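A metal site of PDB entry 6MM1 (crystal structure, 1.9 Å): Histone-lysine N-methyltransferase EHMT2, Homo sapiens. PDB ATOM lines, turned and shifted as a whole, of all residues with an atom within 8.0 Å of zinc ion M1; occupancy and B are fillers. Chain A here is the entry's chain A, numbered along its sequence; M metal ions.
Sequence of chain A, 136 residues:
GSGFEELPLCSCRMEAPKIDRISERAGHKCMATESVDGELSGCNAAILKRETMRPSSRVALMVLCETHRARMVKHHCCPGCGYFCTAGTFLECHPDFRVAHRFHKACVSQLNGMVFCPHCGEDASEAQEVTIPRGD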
ATOM      1  N   LEU A   9      -1.454 -15.066  25.920  1.00  0.00           N
ATOM      2  CA  LEU A   9      -1.669 -16.317  25.204  1.00  0.00           C
ATOM      3  C   LEU A   9      -2.811 -16.113  24.215  1.00  0.00           C
ATOM      4  O   LEU A   9      -3.678 -15.262  24.421  1.00  0.00           O
ATOM      5  CB  LEU A   9      -2.007 -17.455  26.188  1.00  0.00           C
ATOM      6  CG  LEU A   9      -1.028 -17.611  27.357  1.00  0.00           C
ATOM      7  CD1 LEU A   9      -1.519 -18.674  28.335  1.00  0.00           C
ATOM      8  CD2 LEU A   9       0.365 -17.956  26.857  1.00  0.00           C
ATOM      9  N   CYS A  10      -2.812 -16.897  23.140  1.00  0.00           N
ATOM     10  CA  CYS A  10      -3.740 -16.666  22.046  1.00  0.00           C
ATOM     11  C   CYS A  10      -5.131 -17.161  22.386  1.00  0.00           C
ATOM     12  O   CYS A  10      -5.332 -17.925  23.324  1.00  0.00           O
ATOM     13  CB  CYS A  10      -3.262 -17.370  20.771  1.00  0.00           C
ATOM     14  SG  CYS A  10      -3.301 -19.201  20.949  1.00  0.00           S
ATOM     15  N   SER A  11      -6.116 -16.741  21.571  1.00  0.00           N
ATOM     16  CA  SER A  11      -7.505 -17.150  21.715  1.00  0.00           C
ATOM     17  C   SER A  11      -7.970 -17.970  20.519  1.00  0.00           C
ATOM     18  O   SER A  11      -9.169 -18.051  20.241  1.00  0.00           O
ATOM     19  CB  SER A  11      -8.401 -15.917  21.907  1.00  0.00           C
ATOM     20  OG  SER A  11      -8.361 -15.098  20.752  1.00  0.00           O
ATOM     21  N   CYS A  12      -7.025 -18.586  19.815  1.00  0.00           N
ATOM     22  CA  CYS A  12      -7.318 -19.299  18.567  1.00  0.00           C
ATOM     23  C   CYS A  12      -8.356 -20.408  18.766  1.00  0.00           C
ATOM     24  O   CYS A  12      -9.072 -20.753  17.815  1.00  0.00           O
ATOM     25  CB  CYS A  12      -6.033 -19.912  17.998  1.00  0.00           C
ATOM     26  SG  CYS A  12      -4.736 -18.677  17.662  1.00  0.00           S
ATOM     27  N   ARG A  13      -8.429 -21.001  19.953  1.00  0.00           N
ATOM     28  CA  ARG A  13      -9.359 -22.097  20.191  1.00  0.00           C
ATOM     29  C   ARG A  13     -10.682 -21.636  20.812  1.00  0.00           C
ATOM     30  O   ARG A  13     -11.544 -22.474  21.075  1.00  0.00           O
ATOM     31  CB  ARG A  13      -8.711 -23.149  21.095  1.00  0.00           C
ATOM     32  CG  ARG A  13      -7.398 -23.739  20.545  1.00  0.00           C
ATOM     33  CD  ARG A  13      -7.620 -25.066  19.810  1.00  0.00           C
ATOM     34  NE  ARG A  13      -6.424 -25.548  19.109  1.00  0.00           N
ATOM     35  CZ  ARG A  13      -5.684 -26.581  19.500  1.00  0.00           C
ATOM     36  NH1 ARG A  13      -5.978 -27.264  20.608  1.00  0.00           N
ATOM     37  NH2 ARG A  13      -4.636 -26.947  18.786  1.00  0.00           N
ATOM     38  N   ARG A  54     -11.098 -15.328  16.685  1.00  0.00           N
ATOM     39  CA  ARG A  54      -9.960 -14.437  16.470  1.00  0.00           C
ATOM     40  C   ARG A  54      -8.768 -14.984  17.234  1.00  0.00           C
ATOM     41  O   ARG A  54      -8.946 -15.626  18.276  1.00  0.00           O
ATOM     42  CB  ARG A  54     -10.282 -13.021  16.944  1.00  0.00           C
ATOM     43  CG  ARG A  54     -10.587 -12.913  18.413  1.00  0.00           C
ATOM     44  CD  ARG A  54     -11.059 -11.526  18.734  1.00  0.00           C
ATOM     45  NE  ARG A  54     -11.473 -11.373  20.114  1.00  0.00           N
ATOM     46  CZ  ARG A  54     -11.932 -10.233  20.608  1.00  0.00           C
ATOM     47  NH1 ARG A  54     -12.037  -9.168  19.816  1.00  0.00           N
ATOM     48  NH2 ARG A  54     -12.285 -10.161  21.885  1.00  0.00           N
ATOM     49  N   PRO A  55      -7.534 -14.745  16.757  1.00  0.00           N
ATOM     50  CA  PRO A  55      -6.360 -15.315  17.441  1.00  0.00           C
ATOM     51  C   PRO A  55      -5.986 -14.559  18.700  1.00  0.00           C
ATOM     52  O   PRO A  55      -5.306 -15.116  19.568  1.00  0.00           O
ATOM     53  CB  PRO A  55      -5.252 -15.210  16.393  1.00  0.00           C
ATOM     54  CG  PRO A  55      -5.645 -14.005  15.571  1.00  0.00           C
ATOM     55  CD  PRO A  55      -7.165 -13.997  15.543  1.00  0.00           C
ATOM     56  N   SER A  56      -6.386 -13.295  18.804  1.00  0.00           N
ATOM     57  CA  SER A  56      -6.185 -12.525  20.022  1.00  0.00           C
ATOM     58  C   SER A  56      -7.173 -11.365  19.994  1.00  0.00           C
ATOM     59  O   SER A  56      -7.795 -11.082  18.962  1.00  0.00           O
ATOM     60  CB  SER A  56      -4.749 -12.007  20.131  1.00  0.00           C
ATOM     61  OG  SER A  56      -4.608 -10.784  19.429  1.00  0.00           O
ATOM     62  N   ARG A  71      -7.926 -23.822   9.985  1.00  0.00           N
ATOM     63  CA  ARG A  71      -6.569 -23.280  10.102  1.00  0.00           C
ATOM     64  C   ARG A  71      -6.413 -22.482  11.393  1.00  0.00           C
ATOM     65  O   ARG A  71      -5.363 -22.512  12.040  1.00  0.00           O
ATOM     66  CB  ARG A  71      -6.228 -22.446   8.872  1.00  0.00           C
ATOM     67  CG  ARG A  71      -6.095 -23.276   7.604  1.00  0.00           C
ATOM     68  CD  ARG A  71      -5.862 -22.404   6.398  1.00  0.00           C
ATOM     69  NE  ARG A  71      -5.849 -23.190   5.162  1.00  0.00           N
ATOM     70  CZ  ARG A  71      -6.042 -22.673   3.951  1.00  0.00           C
ATOM     71  NH1 ARG A  71      -6.244 -21.369   3.813  1.00  0.00           N
ATOM     72  NH2 ARG A  71      -6.025 -23.463   2.889  1.00  0.00           N
ATOM     73  N   MET A  72      -7.471 -21.776  11.807  1.00  0.00           N
ATOM     74  CA  MET A  72      -7.411 -21.000  13.032  1.00  0.00           C
ATOM     75  C   MET A  72      -7.129 -21.894  14.241  1.00  0.00           C
ATOM     76  O   MET A  72      -6.256 -21.586  15.070  1.00  0.00           O
ATOM     77  CB  MET A  72      -8.725 -20.233  13.228  1.00  0.00           C
ATOM     78  CG  MET A  72      -8.858 -19.591  14.567  1.00  0.00           C
ATOM     79  SD  MET A  72      -8.061 -17.972  14.578  1.00  0.00           S
ATOM     80  CE  MET A  72      -9.002 -17.040  13.359  1.00  0.00           C
ATOM     81  N   VAL A  73      -7.835 -23.024  14.353  1.00  0.00           N
ATOM     82  CA  VAL A  73      -7.619 -23.849  15.534  1.00  0.00           C
ATOM     83  C   VAL A  73      -6.277 -24.550  15.534  1.00  0.00           C
ATOM     84  O   VAL A  73      -5.834 -25.028  16.580  1.00  0.00           O
ATOM     85  CB  VAL A  73      -8.751 -24.899  15.714  1.00  0.00           C
ATOM     86  CG1 VAL A  73     -10.075 -24.202  15.931  1.00  0.00           C
ATOM     87  CG2 VAL A  73      -8.820 -25.840  14.536  1.00  0.00           C
ATOM     88  N   LYS A  74      -5.601 -24.635  14.383  1.00  0.00           N
ATOM     89  CA  LYS A  74      -4.228 -25.148  14.325  1.00  0.00           C
ATOM     90  C   LYS A  74      -3.185 -24.089  14.643  1.00  0.00           C
ATOM     91  O   LYS A  74      -1.990 -24.371  14.510  1.00  0.00           O
ATOM     92  CB  LYS A  74      -3.925 -25.716  12.929  1.00  0.00           C
ATOM     93  CG  LYS A  74      -4.757 -26.928  12.544  1.00  0.00           C
ATOM     94  CD  LYS A  74      -4.650 -27.184  11.049  1.00  0.00           C
ATOM     95  CE  LYS A  74      -3.896 -28.457  10.757  1.00  0.00           C
ATOM     96  NZ  LYS A  74      -4.647 -29.344   9.809  1.00  0.00           N
ATOM     97  N   HIS A  75      -3.597 -22.891  15.062  1.00  0.00           N
ATOM     98  CA  HIS A  75      -2.701 -21.791  15.380  1.00  0.00           C
ATOM     99  C   HIS A  75      -1.939 -21.321  14.148  1.00  0.00           C
ATOM    100  O   HIS A  75      -0.777 -20.954  14.223  1.00  0.00           O
ATOM    101  CB  HIS A  75      -1.738 -22.164  16.511  1.00  0.00           C
ATOM    102  CG  HIS A  75      -2.423 -22.529  17.795  1.00  0.00           C
ATOM    103  ND1 HIS A  75      -3.104 -21.612  18.568  1.00  0.00           N
ATOM    104  CD2 HIS A  75      -2.538 -23.716  18.432  1.00  0.00           C
ATOM    105  CE1 HIS A  75      -3.599 -22.215  19.634  1.00  0.00           C
ATOM    106  NE2 HIS A  75      -3.256 -23.493  19.577  1.00  0.00           N
ATOM    107  N   HIS A  76      -2.605 -21.330  12.985  1.00  0.00           N
ATOM    108  CA  HIS A  76      -1.999 -20.837  11.764  1.00  0.00           C
ATOM    109  C   HIS A  76      -2.318 -19.368  11.487  1.00  0.00           C
ATOM    110  O   HIS A  76      -1.824 -18.809  10.510  1.00  0.00           O
ATOM    111  CB  HIS A  76      -2.439 -21.677  10.574  1.00  0.00           C
ATOM    112  CG  HIS A  76      -1.800 -23.025  10.528  1.00  0.00           C
ATOM    113  ND1 HIS A  76      -1.962 -23.900   9.482  1.00  0.00           N
ATOM    114  CD2 HIS A  76      -0.996 -23.641  11.428  1.00  0.00           C
ATOM    115  CE1 HIS A  76      -1.281 -25.002   9.726  1.00  0.00           C
ATOM    116  NE2 HIS A  76      -0.688 -24.874  10.893  1.00  0.00           N
ATOM    117  N   CYS A  77      -3.113 -18.721  12.343  1.00  0.00           N
ATOM    118  CA  CYS A  77      -3.414 -17.307  12.219  1.00  0.00           C
ATOM    119  C   CYS A  77      -2.540 -16.534  13.198  1.00  0.00           C
ATOM    120  O   CYS A  77      -2.349 -16.949  14.342  1.00  0.00           O
ATOM    121  CB  CYS A  77      -4.895 -17.048  12.511  1.00  0.00           C
ATOM    122  SG  CYS A  77      -5.424 -15.379  12.069  1.00  0.00           S
ATOM    123  N   CYS A  78      -1.990 -15.412  12.746  1.00  0.00           N
ATOM    124  CA  CYS A  78      -1.058 -14.658  13.591  1.00  0.00           C
ATOM    125  C   CYS A  78      -1.810 -13.872  14.663  1.00  0.00           C
ATOM    126  O   CYS A  78      -2.643 -13.023  14.323  1.00  0.00           O
ATOM    127  CB  CYS A  78      -0.209 -13.709  12.749  1.00  0.00           C
ATOM    128  SG  CYS A  78       1.068 -12.911  13.722  1.00  0.00           S
ATOM    129  N   PRO A  79      -1.516 -14.085  15.947  1.00  0.00           N
ATOM    130  CA  PRO A  79      -2.179 -13.286  16.985  1.00  0.00           C
ATOM    131  C   PRO A  79      -1.773 -11.833  16.965  1.00  0.00           C
ATOM    132  O   PRO A  79      -2.482 -11.002  17.556  1.00  0.00           O
ATOM    133  CB  PRO A  79      -1.730 -13.965  18.298  1.00  0.00           C
ATOM    134  CG  PRO A  79      -1.142 -15.291  17.887  1.00  0.00           C
ATOM    135  CD  PRO A  79      -0.587 -15.068  16.511  1.00  0.00           C
ATOM    136  N   ALA A 100       2.375 -26.710  15.120  1.00  0.00           N
ATOM    137  CA  ALA A 100       3.086 -25.513  14.671  1.00  0.00           C
ATOM    138  C   ALA A 100       2.268 -24.293  15.026  1.00  0.00           C
ATOM    139  O   ALA A 100       1.096 -24.211  14.654  1.00  0.00           O
ATOM    140  CB  ALA A 100       3.327 -25.555  13.155  1.00  0.00           C
ATOM    141  N   HIS A 101       2.872 -23.369  15.761  1.00  0.00           N
ATOM    142  CA  HIS A 101       2.307 -22.050  16.013  1.00  0.00           C
ATOM    143  C   HIS A 101       2.945 -21.082  15.035  1.00  0.00           C
ATOM    144  O   HIS A 101       4.167 -20.873  15.090  1.00  0.00           O
ATOM    145  CB  HIS A 101       2.600 -21.610  17.447  1.00  0.00           C
ATOM    146  CG  HIS A 101       2.055 -22.532  18.498  1.00  0.00           C
ATOM    147  ND1 HIS A 101       2.546 -22.555  19.781  1.00  0.00           N
ATOM    148  CD2 HIS A 101       1.043 -23.429  18.461  1.00  0.00           C
ATOM    149  CE1 HIS A 101       1.874 -23.441  20.498  1.00  0.00           C
ATOM    150  NE2 HIS A 101       0.953 -23.985  19.712  1.00  0.00           N
ATOM    151  N   ARG A 102       2.152 -20.491  14.140  1.00  0.00           N
ATOM    152  CA  ARG A 102       2.694 -19.655  13.092  1.00  0.00           C
ATOM    153  C   ARG A 102       2.506 -18.199  13.450  1.00  0.00           C
ATOM    154  O   ARG A 102       1.458 -17.800  13.976  1.00  0.00           O
ATOM    155  CB  ARG A 102       2.035 -19.940  11.740  1.00  0.00           C
ATOM    156  CG  ARG A 102       2.168 -21.364  11.270  1.00  0.00           C
ATOM    157  CD  ARG A 102       1.584 -21.533   9.876  1.00  0.00           C
ATOM    158  NE  ARG A 102       1.903 -22.848   9.335  1.00  0.00           N
ATOM    159  CZ  ARG A 102       1.444 -23.314   8.185  1.00  0.00           C
ATOM    160  NH1 ARG A 102       0.617 -22.581   7.447  1.00  0.00           N
ATOM    161  NH2 ARG A 102       1.789 -24.536   7.784  1.00  0.00           N
ATOM    162  N   CYS A 117       6.743 -16.612  21.598  1.00  0.00           N
ATOM    163  CA  CYS A 117       5.667 -17.036  20.716  1.00  0.00           C
ATOM    164  C   CYS A 117       4.375 -16.380  21.166  1.00  0.00           C
ATOM    165  O   CYS A 117       4.008 -16.488  22.348  1.00  0.00           O
ATOM    166  CB  CYS A 117       5.524 -18.570  20.724  1.00  0.00           C
ATOM    167  SG  CYS A 117       4.064 -19.229  19.812  1.00  0.00           S
ATOM    168  N   PRO A 118       3.657 -15.677  20.291  1.00  0.00           N
ATOM    169  CA  PRO A 118       2.398 -15.039  20.696  1.00  0.00           C
ATOM    170  C   PRO A 118       1.248 -16.007  20.861  1.00  0.00           C
ATOM    171  O   PRO A 118       0.152 -15.573  21.234  1.00  0.00           O
ATOM    172  CB  PRO A 118       2.121 -14.051  19.564  1.00  0.00           C
ATOM    173  CG  PRO A 118       2.730 -14.689  18.393  1.00  0.00           C
ATOM    174  CD  PRO A 118       3.967 -15.431  18.867  1.00  0.00           C
ATOM    175  N   HIS A 119       1.419 -17.296  20.556  1.00  0.00           N
ATOM    176  CA  HIS A 119       0.365 -18.250  20.901  1.00  0.00           C
ATOM    177  C   HIS A 119       0.540 -18.756  22.322  1.00  0.00           C
ATOM    178  O   HIS A 119      -0.370 -18.620  23.157  1.00  0.00           O
ATOM    179  CB  HIS A 119       0.315 -19.436  19.937  1.00  0.00           C
ATOM    180  CG  HIS A 119       0.119 -19.043  18.501  1.00  0.00           C
ATOM    181  ND1 HIS A 119      -1.123 -19.090  17.899  1.00  0.00           N
ATOM    182  CD2 HIS A 119       0.984 -18.639  17.544  1.00  0.00           C
ATOM    183  CE1 HIS A 119      -1.016 -18.719  16.628  1.00  0.00           C
ATOM    184  NE2 HIS A 119       0.257 -18.445  16.394  1.00  0.00           N
ATOM    185  N   CYS A 120       1.721 -19.331  22.621  1.00  0.00           N
ATOM    186  CA  CYS A 120       1.931 -20.143  23.800  1.00  0.00           C
ATOM    187  C   CYS A 120       2.951 -19.575  24.775  1.00  0.00           C
ATOM    188  O   CYS A 120       3.079 -20.111  25.871  1.00  0.00           O
ATOM    189  CB  CYS A 120       2.385 -21.553  23.399  1.00  0.00           C
ATOM    190  SG  CYS A 120       4.124 -21.622  22.868  1.00  0.00           S
HETATM  191 ZN    ZN M   1      -2.973 -19.698  18.772  1.00  0.00          ZN
HETATM  192 ZN    ZN M   2       4.188 -21.421  20.563  1.00  0.00          ZN
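The backbone carbonyl oxygen (O) of His 75 sits at hydrogen-bond distance from the backbone NH (N) of Arg 102 (3.0 Å).
A ring nitrogen (NE2) of His 119 sits at hydrogen-bond distance from the backbone carbonyl oxygen (O) of Arg 102, at 2.8 Å.
N of His 119 sits close to SG of Cys 117 (3.4 Å).
Zinc ion M1 is bound by ND1 of His 75 (1.9 Å), ND1 of His 119 (2.1 Å), SG of Cys 10 (2.3 Å) and SG of Cys 12 (2.3 Å).
Zinc ion M1 has four donor atoms within binding distance.
Four residues have an atom within 4 Å of zinc ion M1: Cys 10, Cys 12, His 75 and His 119.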
